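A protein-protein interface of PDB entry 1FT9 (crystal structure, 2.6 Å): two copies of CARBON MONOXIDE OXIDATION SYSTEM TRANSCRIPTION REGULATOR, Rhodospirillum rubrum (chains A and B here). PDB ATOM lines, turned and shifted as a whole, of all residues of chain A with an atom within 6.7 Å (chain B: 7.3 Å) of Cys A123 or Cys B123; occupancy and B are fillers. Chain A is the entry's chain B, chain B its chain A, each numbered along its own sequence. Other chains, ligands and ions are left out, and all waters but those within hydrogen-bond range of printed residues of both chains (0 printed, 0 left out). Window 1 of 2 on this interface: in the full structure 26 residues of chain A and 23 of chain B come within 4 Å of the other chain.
Leu A56 touches Ile B127, but with the chains exchanged Ile A127 does not touch Leu B56 (4.5 Å). Cys A123 touches its own counterpart, Cys B123. Cys A123 touches Ile B127, and with the chains exchanged Ile A127 touches Cys B123. Ile B127 touches its own counterpart, Ile A127. 15 positions are printed for both chains. Of the 12 pairs that touch across the chains among the printed residues, 9 have their exchanged pair printed and touching as well.
Among the printed residues, pairs that only touch across the chains: Leu A56 with Ile B127, Ala A119 with Leu B120, Leu A120 with Leu B120, Leu A120 with Cys B123, Cys A123 with Leu B120, Cys A123 with Cys B123, Cys A123 with Ile B127, Ile A127 with Cys B123, Ile A127 with Thr B126 and Ile A127 with Ile B127.
Cys A123 touches just these residues of chain B: Leu B120 (3.8 Å), Cys B123 (3.8 Å) and Ile B127 (3.7 Å). Cys B123 touches just these residues of chain A: Leu A120 (3.8 Å), Cys A123 (3.8 Å) and Ile A127 (3.9 Å). Printed residues of chain A within 4 Å of Met B124: Cys A80. Of the printed residues of chain B, Met A124 touches Cys B80. Of the printed residues of chain A, Leu B120 touches Ala A119 (3.7 Å), Leu A120 (3.8 Å) and Cys A123 (3.8 Å). Of the printed residues of chain B, Cys A80 touches Met B124 (3.6 Å). Printed residues of chain B within 4 Å of Leu A56: Ile B127 (3.8 Å). The nearest residue of chain B that does not touch Cys A123 is Met B124 (4.4 Å). The nearest printed residue of chain B that does not touch Ile A127 is Leu B56 (4.5 Å).
Of the 15 printed residues of chain A, 7 touch a printed residue of chain B. Hydrophobic or aromatic side chains of chain A within 4 Å of the printed part of chain B: Leu A56, Ala A119, Leu A120, Met A124 and Ile A127. Of the 17 printed residues of chain B, 6 touch a printed residue of chain A. Hydrophobic or aromatic side chains of chain B within 4 Å of the printed part of chain A: Leu B120, Met B124 and Ile B127. Among the printed residues, no Asp or Glu carboxylate lies within 4 Å of a Lys or Arg side-chain nitrogen of the other chain.
O of Ala B119 lies within hydrogen-bond range of SG of Cys B123, at 3.4 Å. The side-chain sulfur of Cys A123 sits at hydrogen-bond distance from the backbone carbonyl oxygen of Ala A119.
The side-chain sulfur (SG) of Cys B80 lies within hydrogen-bond range of the side-chain sulfur (SD) of Met A124, at 3.7 Å. SG of Cys A80 lies within hydrogen-bond range of SD of Met B124 (3.6 Å).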
ATOM      1  N   LEU A  56      -9.471 -28.197 -24.089  1.00  0.00           N
ATOM      2  CA  LEU A  56      -9.278 -27.641 -22.769  1.00  0.00           C
ATOM      3  C   LEU A  56      -9.443 -28.802 -21.799  1.00  0.00           C
ATOM      4  O   LEU A  56     -10.247 -29.701 -22.040  1.00  0.00           O
ATOM      5  CB  LEU A  56     -10.345 -26.578 -22.508  1.00  0.00           C
ATOM      6  CG  LEU A  56     -10.610 -25.639 -23.688  1.00  0.00           C
ATOM      7  CD1 LEU A  56     -11.881 -24.854 -23.456  1.00  0.00           C
ATOM      8  CD2 LEU A  56      -9.423 -24.717 -23.887  1.00  0.00           C
ATOM      9  N   LEU A  65     -12.464 -28.657 -28.942  1.00  0.00           N
ATOM     10  CA  LEU A  65     -13.066 -27.431 -29.481  1.00  0.00           C
ATOM     11  C   LEU A  65     -13.162 -27.434 -31.002  1.00  0.00           C
ATOM     12  O   LEU A  65     -14.253 -27.309 -31.561  1.00  0.00           O
ATOM     13  CB  LEU A  65     -12.271 -26.203 -29.018  1.00  0.00           C
ATOM     14  CG  LEU A  65     -12.217 -25.984 -27.503  1.00  0.00           C
ATOM     15  CD1 LEU A  65     -11.445 -24.724 -27.179  1.00  0.00           C
ATOM     16  CD2 LEU A  65     -13.624 -25.877 -26.960  1.00  0.00           C
ATOM     17  N   PHE A  66     -12.009 -27.568 -31.655  1.00  0.00           N
ATOM     18  CA  PHE A  66     -11.928 -27.599 -33.112  1.00  0.00           C
ATOM     19  C   PHE A  66     -10.547 -28.098 -33.510  1.00  0.00           C
ATOM     20  O   PHE A  66      -9.676 -28.257 -32.659  1.00  0.00           O
ATOM     21  CB  PHE A  66     -12.166 -26.204 -33.710  1.00  0.00           C
ATOM     22  CG  PHE A  66     -11.162 -25.162 -33.267  1.00  0.00           C
ATOM     23  CD1 PHE A  66     -11.328 -24.476 -32.064  1.00  0.00           C
ATOM     24  CD2 PHE A  66     -10.046 -24.872 -34.050  1.00  0.00           C
ATOM     25  CE1 PHE A  66     -10.394 -23.520 -31.650  1.00  0.00           C
ATOM     26  CE2 PHE A  66      -9.107 -23.917 -33.637  1.00  0.00           C
ATOM     27  CZ  PHE A  66      -9.286 -23.246 -32.440  1.00  0.00           C
ATOM     28  N   CYS A  80      -5.426 -22.686 -24.657  1.00  0.00           N
ATOM     29  CA  CYS A  80      -5.930 -24.009 -25.008  1.00  0.00           C
ATOM     30  C   CYS A  80      -4.737 -24.923 -25.258  1.00  0.00           C
ATOM     31  O   CYS A  80      -3.641 -24.451 -25.584  1.00  0.00           O
ATOM     32  CB  CYS A  80      -6.756 -23.954 -26.293  1.00  0.00           C
ATOM     33  SG  CYS A  80      -7.955 -22.624 -26.424  1.00  0.00           S
ATOM     34  N   ARG A 118     -13.780 -18.970 -35.972  1.00  0.00           N
ATOM     35  CA  ARG A 118     -13.977 -20.405 -35.870  1.00  0.00           C
ATOM     36  C   ARG A 118     -13.850 -20.839 -34.417  1.00  0.00           C
ATOM     37  O   ARG A 118     -14.607 -21.681 -33.951  1.00  0.00           O
ATOM     38  CB  ARG A 118     -12.920 -21.127 -36.702  1.00  0.00           C
ATOM     39  CG  ARG A 118     -12.970 -22.643 -36.605  1.00  0.00           C
ATOM     40  CD  ARG A 118     -13.219 -23.243 -37.973  1.00  0.00           C
ATOM     41  NE  ARG A 118     -12.049 -23.215 -38.847  1.00  0.00           N
ATOM     42  CZ  ARG A 118     -10.980 -23.978 -38.670  1.00  0.00           C
ATOM     43  NH1 ARG A 118     -10.937 -24.813 -37.643  1.00  0.00           N
ATOM     44  NH2 ARG A 118      -9.979 -23.953 -39.548  1.00  0.00           N
ATOM     45  N   ALA A 119     -12.873 -20.282 -33.711  1.00  0.00           N
ATOM     46  CA  ALA A 119     -12.674 -20.616 -32.312  1.00  0.00           C
ATOM     47  C   ALA A 119     -13.855 -20.069 -31.511  1.00  0.00           C
ATOM     48  O   ALA A 119     -14.389 -20.743 -30.632  1.00  0.00           O
ATOM     49  CB  ALA A 119     -11.385 -20.009 -31.814  1.00  0.00           C
ATOM     50  N   LEU A 120     -14.262 -18.841 -31.821  1.00  0.00           N
ATOM     51  CA  LEU A 120     -15.384 -18.222 -31.129  1.00  0.00           C
ATOM     52  C   LEU A 120     -16.597 -19.115 -31.287  1.00  0.00           C
ATOM     53  O   LEU A 120     -17.265 -19.460 -30.313  1.00  0.00           O
ATOM     54  CB  LEU A 120     -15.692 -16.847 -31.722  1.00  0.00           C
ATOM     55  CG  LEU A 120     -16.993 -16.205 -31.236  1.00  0.00           C
ATOM     56  CD1 LEU A 120     -16.970 -16.148 -29.714  1.00  0.00           C
ATOM     57  CD2 LEU A 120     -17.167 -14.813 -31.819  1.00  0.00           C
ATOM     58  N   THR A 121     -16.869 -19.488 -32.531  1.00  0.00           N
ATOM     59  CA  THR A 121     -18.003 -20.334 -32.854  1.00  0.00           C
ATOM     60  C   THR A 121     -17.918 -21.642 -32.093  1.00  0.00           C
ATOM     61  O   THR A 121     -18.889 -22.063 -31.473  1.00  0.00           O
ATOM     62  CB  THR A 121     -18.073 -20.632 -34.372  1.00  0.00           C
ATOM     63  OG1 THR A 121     -18.426 -19.439 -35.082  1.00  0.00           O
ATOM     64  CG2 THR A 121     -19.115 -21.702 -34.665  1.00  0.00           C
ATOM     65  N   SER A 122     -16.756 -22.283 -32.134  1.00  0.00           N
ATOM     66  CA  SER A 122     -16.589 -23.543 -31.435  1.00  0.00           C
ATOM     67  C   SER A 122     -16.916 -23.412 -29.950  1.00  0.00           C
ATOM     68  O   SER A 122     -17.608 -24.267 -29.386  1.00  0.00           O
ATOM     69  CB  SER A 122     -15.164 -24.055 -31.609  1.00  0.00           C
ATOM     70  OG  SER A 122     -14.915 -24.369 -32.968  1.00  0.00           O
ATOM     71  N   CYS A 123     -16.432 -22.341 -29.324  1.00  0.00           N
ATOM     72  CA  CYS A 123     -16.680 -22.121 -27.905  1.00  0.00           C
ATOM     73  C   CYS A 123     -18.144 -21.885 -27.579  1.00  0.00           C
ATOM     74  O   CYS A 123     -18.625 -22.328 -26.540  1.00  0.00           O
ATOM     75  CB  CYS A 123     -15.849 -20.951 -27.394  1.00  0.00           C
ATOM     76  SG  CYS A 123     -14.117 -21.329 -27.385  1.00  0.00           S
ATOM     77  N   MET A 124     -18.858 -21.189 -28.452  1.00  0.00           N
ATOM     78  CA  MET A 124     -20.264 -20.945 -28.190  1.00  0.00           C
ATOM     79  C   MET A 124     -21.056 -22.245 -28.293  1.00  0.00           C
ATOM     80  O   MET A 124     -22.069 -22.427 -27.621  1.00  0.00           O
ATOM     81  CB  MET A 124     -20.820 -19.910 -29.160  1.00  0.00           C
ATOM     82  CG  MET A 124     -20.494 -18.490 -28.776  1.00  0.00           C
ATOM     83  SD  MET A 124     -21.481 -17.347 -29.731  1.00  0.00           S
ATOM     84  CE  MET A 124     -20.208 -16.473 -30.611  1.00  0.00           C
ATOM     85  N   ARG A 125     -20.586 -23.148 -29.141  1.00  0.00           N
ATOM     86  CA  ARG A 125     -21.234 -24.431 -29.316  1.00  0.00           C
ATOM     87  C   ARG A 125     -20.945 -25.241 -28.054  1.00  0.00           C
ATOM     88  O   ARG A 125     -21.837 -25.892 -27.513  1.00  0.00           O
ATOM     89  CB  ARG A 125     -20.667 -25.130 -30.565  1.00  0.00           C
ATOM     90  CG  ARG A 125     -20.466 -26.644 -30.438  1.00  0.00           C
ATOM     91  CD  ARG A 125     -19.404 -27.147 -31.429  1.00  0.00           C
ATOM     92  NE  ARG A 125     -19.073 -28.569 -31.269  1.00  0.00           N
ATOM     93  CZ  ARG A 125     -18.259 -29.068 -30.339  1.00  0.00           C
ATOM     94  NH1 ARG A 125     -17.671 -28.268 -29.459  1.00  0.00           N
ATOM     95  NH2 ARG A 125     -18.027 -30.377 -30.289  1.00  0.00           N
ATOM     96  N   THR A 126     -19.700 -25.176 -27.584  1.00  0.00           N
ATOM     97  CA  THR A 126     -19.277 -25.909 -26.391  1.00  0.00           C
ATOM     98  C   THR A 126     -20.028 -25.475 -25.145  1.00  0.00           C
ATOM     99  O   THR A 126     -20.285 -26.277 -24.246  1.00  0.00           O
ATOM    100  CB  THR A 126     -17.781 -25.724 -26.110  1.00  0.00           C
ATOM    101  OG1 THR A 126     -17.022 -26.219 -27.217  1.00  0.00           O
ATOM    102  CG2 THR A 126     -17.383 -26.483 -24.844  1.00  0.00           C
ATOM    103  N   ILE A 127     -20.359 -24.195 -25.080  1.00  0.00           N
ATOM    104  CA  ILE A 127     -21.095 -23.687 -23.941  1.00  0.00           C
ATOM    105  C   ILE A 127     -22.518 -24.242 -24.022  1.00  0.00           C
ATOM    106  O   ILE A 127     -23.071 -24.695 -23.020  1.00  0.00           O
ATOM    107  CB  ILE A 127     -21.094 -22.137 -23.937  1.00  0.00           C
ATOM    108  CG1 ILE A 127     -19.680 -21.633 -23.634  1.00  0.00           C
ATOM    109  CG2 ILE A 127     -22.084 -21.606 -22.924  1.00  0.00           C
ATOM    110  CD1 ILE A 127     -19.484 -20.144 -23.892  1.00  0.00           C
ATOM    111  N   GLU A 128     -23.102 -24.228 -25.215  1.00  0.00           N
ATOM    112  CA  GLU A 128     -24.452 -24.749 -25.386  1.00  0.00           C
ATOM    113  C   GLU A 128     -24.508 -26.216 -24.976  1.00  0.00           C
ATOM    114  O   GLU A 128     -25.484 -26.662 -24.374  1.00  0.00           O
ATOM    115  CB  GLU A 128     -24.911 -24.611 -26.838  1.00  0.00           C
ATOM    116  CG  GLU A 128     -25.203 -23.183 -27.265  1.00  0.00           C
ATOM    117  CD  GLU A 128     -25.692 -23.090 -28.707  1.00  0.00           C
ATOM    118  OE1 GLU A 128     -24.926 -23.467 -29.624  1.00  0.00           O
ATOM    119  OE2 GLU A 128     -26.842 -22.641 -28.924  1.00  0.00           O
ATOM    120  N   LEU B  56     -25.282 -14.459 -23.309  1.00  0.00           N
ATOM    121  CA  LEU B  56     -26.014 -15.674 -23.618  1.00  0.00           C
ATOM    122  C   LEU B  56     -26.754 -15.970 -22.316  1.00  0.00           C
ATOM    123  O   LEU B  56     -26.392 -15.438 -21.263  1.00  0.00           O
ATOM    124  CB  LEU B  56     -25.037 -16.809 -23.938  1.00  0.00           C
ATOM    125  CG  LEU B  56     -24.131 -16.616 -25.155  1.00  0.00           C
ATOM    126  CD1 LEU B  56     -23.014 -17.649 -25.146  1.00  0.00           C
ATOM    127  CD2 LEU B  56     -24.965 -16.719 -26.422  1.00  0.00           C
ATOM    128  N   LEU B  65     -20.932 -11.906 -21.264  1.00  0.00           N
ATOM    129  CA  LEU B  65     -19.657 -12.170 -21.908  1.00  0.00           C
ATOM    130  C   LEU B  65     -18.729 -10.971 -21.818  1.00  0.00           C
ATOM    131  O   LEU B  65     -17.641 -11.067 -21.250  1.00  0.00           O
ATOM    132  CB  LEU B  65     -19.885 -12.580 -23.364  1.00  0.00           C
ATOM    133  CG  LEU B  65     -20.652 -13.898 -23.521  1.00  0.00           C
ATOM    134  CD1 LEU B  65     -20.963 -14.131 -24.984  1.00  0.00           C
ATOM    135  CD2 LEU B  65     -19.834 -15.061 -22.951  1.00  0.00           C
ATOM    136  N   PHE B  66     -19.159  -9.843 -22.377  1.00  0.00           N
ATOM    137  CA  PHE B  66     -18.362  -8.618 -22.348  1.00  0.00           C
ATOM    138  C   PHE B  66     -19.238  -7.429 -22.691  1.00  0.00           C
ATOM    139  O   PHE B  66     -20.436  -7.577 -22.934  1.00  0.00           O
ATOM    140  CB  PHE B  66     -17.183  -8.691 -23.341  1.00  0.00           C
ATOM    141  CG  PHE B  66     -17.594  -8.975 -24.765  1.00  0.00           C
ATOM    142  CD1 PHE B  66     -17.797 -10.283 -25.201  1.00  0.00           C
ATOM    143  CD2 PHE B  66     -17.796  -7.932 -25.668  1.00  0.00           C
ATOM    144  CE1 PHE B  66     -18.195 -10.549 -26.524  1.00  0.00           C
ATOM    145  CE2 PHE B  66     -18.196  -8.192 -26.986  1.00  0.00           C
ATOM    146  CZ  PHE B  66     -18.393  -9.502 -27.410  1.00  0.00           C
ATOM    147  N   CYS B  80     -25.138 -13.930 -30.498  1.00  0.00           N
ATOM    148  CA  CYS B  80     -25.079 -13.397 -29.149  1.00  0.00           C
ATOM    149  C   CYS B  80     -26.188 -12.373 -28.952  1.00  0.00           C
ATOM    150  O   CYS B  80     -26.736 -11.831 -29.916  1.00  0.00           O
ATOM    151  CB  CYS B  80     -23.728 -12.725 -28.898  1.00  0.00           C
ATOM    152  SG  CYS B  80     -22.356 -13.856 -28.686  1.00  0.00           S
ATOM    153  N   GLY B 117     -11.250 -11.411 -30.386  1.00  0.00           N
ATOM    154  CA  GLY B 117     -10.440 -11.934 -29.307  1.00  0.00           C
ATOM    155  C   GLY B 117     -11.150 -11.728 -27.978  1.00  0.00           C
ATOM    156  O   GLY B 117     -11.215 -12.640 -27.136  1.00  0.00           O
ATOM    157  N   ARG B 118     -11.691 -10.529 -27.778  1.00  0.00           N
ATOM    158  CA  ARG B 118     -12.396 -10.249 -26.542  1.00  0.00           C
ATOM    159  C   ARG B 118     -13.550 -11.237 -26.398  1.00  0.00           C
ATOM    160  O   ARG B 118     -13.752 -11.834 -25.335  1.00  0.00           O
ATOM    161  CB  ARG B 118     -12.942  -8.828 -26.529  1.00  0.00           C
ATOM    162  CG  ARG B 118     -13.462  -8.433 -25.156  1.00  0.00           C
ATOM    163  CD  ARG B 118     -14.184  -7.100 -25.168  1.00  0.00           C
ATOM    164  NE  ARG B 118     -13.359  -6.020 -25.693  1.00  0.00           N
ATOM    165  CZ  ARG B 118     -13.816  -4.790 -25.906  1.00  0.00           C
ATOM    166  NH1 ARG B 118     -15.081  -4.504 -25.636  1.00  0.00           N
ATOM    167  NH2 ARG B 118     -13.014  -3.843 -26.392  1.00  0.00           N
ATOM    168  N   ALA B 119     -14.299 -11.421 -27.477  1.00  0.00           N
ATOM    169  CA  ALA B 119     -15.425 -12.340 -27.457  1.00  0.00           C
ATOM    170  C   ALA B 119     -14.944 -13.747 -27.158  1.00  0.00           C
ATOM    171  O   ALA B 119     -15.554 -14.460 -26.369  1.00  0.00           O
ATOM    172  CB  ALA B 119     -16.150 -12.317 -28.801  1.00  0.00           C
ATOM    173  N   LEU B 120     -13.845 -14.146 -27.786  1.00  0.00           N
ATOM    174  CA  LEU B 120     -13.319 -15.487 -27.581  1.00  0.00           C
ATOM    175  C   LEU B 120     -12.924 -15.766 -26.130  1.00  0.00           C
ATOM    176  O   LEU B 120     -13.439 -16.709 -25.524  1.00  0.00           O
ATOM    177  CB  LEU B 120     -12.121 -15.738 -28.499  1.00  0.00           C
ATOM    178  CG  LEU B 120     -11.405 -17.083 -28.332  1.00  0.00           C
ATOM    179  CD1 LEU B 120     -12.373 -18.219 -28.627  1.00  0.00           C
ATOM    180  CD2 LEU B 120     -10.221 -17.163 -29.262  1.00  0.00           C
ATOM    181  N   THR B 121     -12.021 -14.952 -25.570  1.00  0.00           N
ATOM    182  CA  THR B 121     -11.570 -15.169 -24.193  1.00  0.00           C
ATOM    183  C   THR B 121     -12.756 -15.113 -23.226  1.00  0.00           C
ATOM    184  O   THR B 121     -12.806 -15.864 -22.261  1.00  0.00           O
ATOM    185  CB  THR B 121     -10.454 -14.155 -23.743  1.00  0.00           C
ATOM    186  OG1 THR B 121     -11.043 -13.047 -23.068  1.00  0.00           O
ATOM    187  CG2 THR B 121      -9.665 -13.646 -24.929  1.00  0.00           C
ATOM    188  N   SER B 122     -13.722 -14.244 -23.487  1.00  0.00           N
ATOM    189  CA  SER B 122     -14.889 -14.186 -22.618  1.00  0.00           C
ATOM    190  C   SER B 122     -15.480 -15.582 -22.554  1.00  0.00           C
ATOM    191  O   SER B 122     -15.720 -16.107 -21.470  1.00  0.00           O
ATOM    192  CB  SER B 122     -15.948 -13.234 -23.171  1.00  0.00           C
ATOM    193  OG  SER B 122     -15.518 -11.889 -23.067  1.00  0.00           O
ATOM    194  N   CYS B 123     -15.708 -16.176 -23.723  1.00  0.00           N
ATOM    195  CA  CYS B 123     -16.280 -17.511 -23.823  1.00  0.00           C
ATOM    196  C   CYS B 123     -15.406 -18.563 -23.148  1.00  0.00           C
ATOM    197  O   CYS B 123     -15.904 -19.488 -22.511  1.00  0.00           O
ATOM    198  CB  CYS B 123     -16.485 -17.895 -25.292  1.00  0.00           C
ATOM    199  SG  CYS B 123     -17.782 -16.976 -26.127  1.00  0.00           S
ATOM    200  N   MET B 124     -14.100 -18.438 -23.300  1.00  0.00           N
ATOM    201  CA  MET B 124     -13.209 -19.398 -22.677  1.00  0.00           C
ATOM    202  C   MET B 124     -13.392 -19.298 -21.176  1.00  0.00           C
ATOM    203  O   MET B 124     -13.438 -20.303 -20.466  1.00  0.00           O
ATOM    204  CB  MET B 124     -11.778 -19.080 -23.053  1.00  0.00           C
ATOM    205  CG  MET B 124     -11.579 -19.092 -24.534  1.00  0.00           C
ATOM    206  SD  MET B 124     -10.354 -20.294 -24.995  1.00  0.00           S
ATOM    207  CE  MET B 124      -8.948 -19.212 -25.346  1.00  0.00           C
ATOM    208  N   ARG B 125     -13.512 -18.070 -20.699  1.00  0.00           N
ATOM    209  CA  ARG B 125     -13.698 -17.844 -19.287  1.00  0.00           C
ATOM    210  C   ARG B 125     -14.986 -18.516 -18.841  1.00  0.00           C
ATOM    211  O   ARG B 125     -14.999 -19.200 -17.829  1.00  0.00           O
ATOM    212  CB  ARG B 125     -13.758 -16.347 -19.007  1.00  0.00           C
ATOM    213  CG  ARG B 125     -14.220 -15.993 -17.614  1.00  0.00           C
ATOM    214  CD  ARG B 125     -15.066 -14.750 -17.671  1.00  0.00           C
ATOM    215  NE  ARG B 125     -14.401 -13.735 -18.481  1.00  0.00           N
ATOM    216  CZ  ARG B 125     -15.036 -12.800 -19.177  1.00  0.00           C
ATOM    217  NH1 ARG B 125     -16.362 -12.747 -19.158  1.00  0.00           N
ATOM    218  NH2 ARG B 125     -14.344 -11.935 -19.905  1.00  0.00           N
ATOM    219  N   THR B 126     -16.066 -18.328 -19.597  1.00  0.00           N
ATOM    220  CA  THR B 126     -17.351 -18.925 -19.251  1.00  0.00           C
ATOM    221  C   THR B 126     -17.295 -20.461 -19.270  1.00  0.00           C
ATOM    222  O   THR B 126     -17.915 -21.121 -18.433  1.00  0.00           O
ATOM    223  CB  THR B 126     -18.465 -18.414 -20.195  1.00  0.00           C
ATOM    224  OG1 THR B 126     -18.809 -17.068 -19.831  1.00  0.00           O
ATOM    225  CG2 THR B 126     -19.715 -19.284 -20.090  1.00  0.00           C
ATOM    226  N   ILE B 127     -16.552 -21.019 -20.222  1.00  0.00           N
ATOM    227  CA  ILE B 127     -16.385 -22.466 -20.329  1.00  0.00           C
ATOM    228  C   ILE B 127     -15.568 -22.937 -19.126  1.00  0.00           C
ATOM    229  O   ILE B 127     -15.833 -23.995 -18.543  1.00  0.00           O
ATOM    230  CB  ILE B 127     -15.603 -22.851 -21.616  1.00  0.00           C
ATOM    231  CG1 ILE B 127     -16.486 -22.638 -22.850  1.00  0.00           C
ATOM    232  CG2 ILE B 127     -15.080 -24.301 -21.519  1.00  0.00           C
ATOM    233  CD1 ILE B 127     -15.732 -22.835 -24.169  1.00  0.00           C
ATOM    234  N   GLU B 128     -14.565 -22.138 -18.773  1.00  0.00           N
ATOM    235  CA  GLU B 128     -13.680 -22.440 -17.657  1.00  0.00           C
ATOM    236  C   GLU B 128     -14.470 -22.412 -16.353  1.00  0.00           C
ATOM    237  O   GLU B 128     -14.203 -23.193 -15.441  1.00  0.00           O
ATOM    238  CB  GLU B 128     -12.539 -21.418 -17.607  1.00  0.00           C
ATOM    239  CG  GLU B 128     -11.493 -21.697 -16.545  1.00  0.00           C
ATOM    240  CD  GLU B 128     -10.640 -20.481 -16.219  1.00  0.00           C
ATOM    241  OE1 GLU B 128     -11.208 -19.435 -15.816  1.00  0.00           O
ATOM    242  OE2 GLU B 128      -9.399 -20.580 -16.359  1.00  0.00           O
ATOM    243  N   ASP B 129     -15.450 -21.517 -16.270  1.00  0.00           N
ATOM    244  CA  ASP B 129     -16.268 -21.414 -15.068  1.00  0.00           C
ATOM    245  C   ASP B 129     -17.144 -22.648 -14.893  1.00  0.00           C
ATOM    246  O   ASP B 129     -17.549 -22.966 -13.784  1.00  0.00           O
ATOM    247  CB  ASP B 129     -17.175 -20.169 -15.102  1.00  0.00           C
ATOM    248  CG  ASP B 129     -16.391 -18.848 -15.078  1.00  0.00           C
ATOM    249  OD1 ASP B 129     -15.175 -18.851 -14.759  1.00  0.00           O
ATOM    250  OD2 ASP B 129     -17.011 -17.796 -15.372  1.00  0.00           O
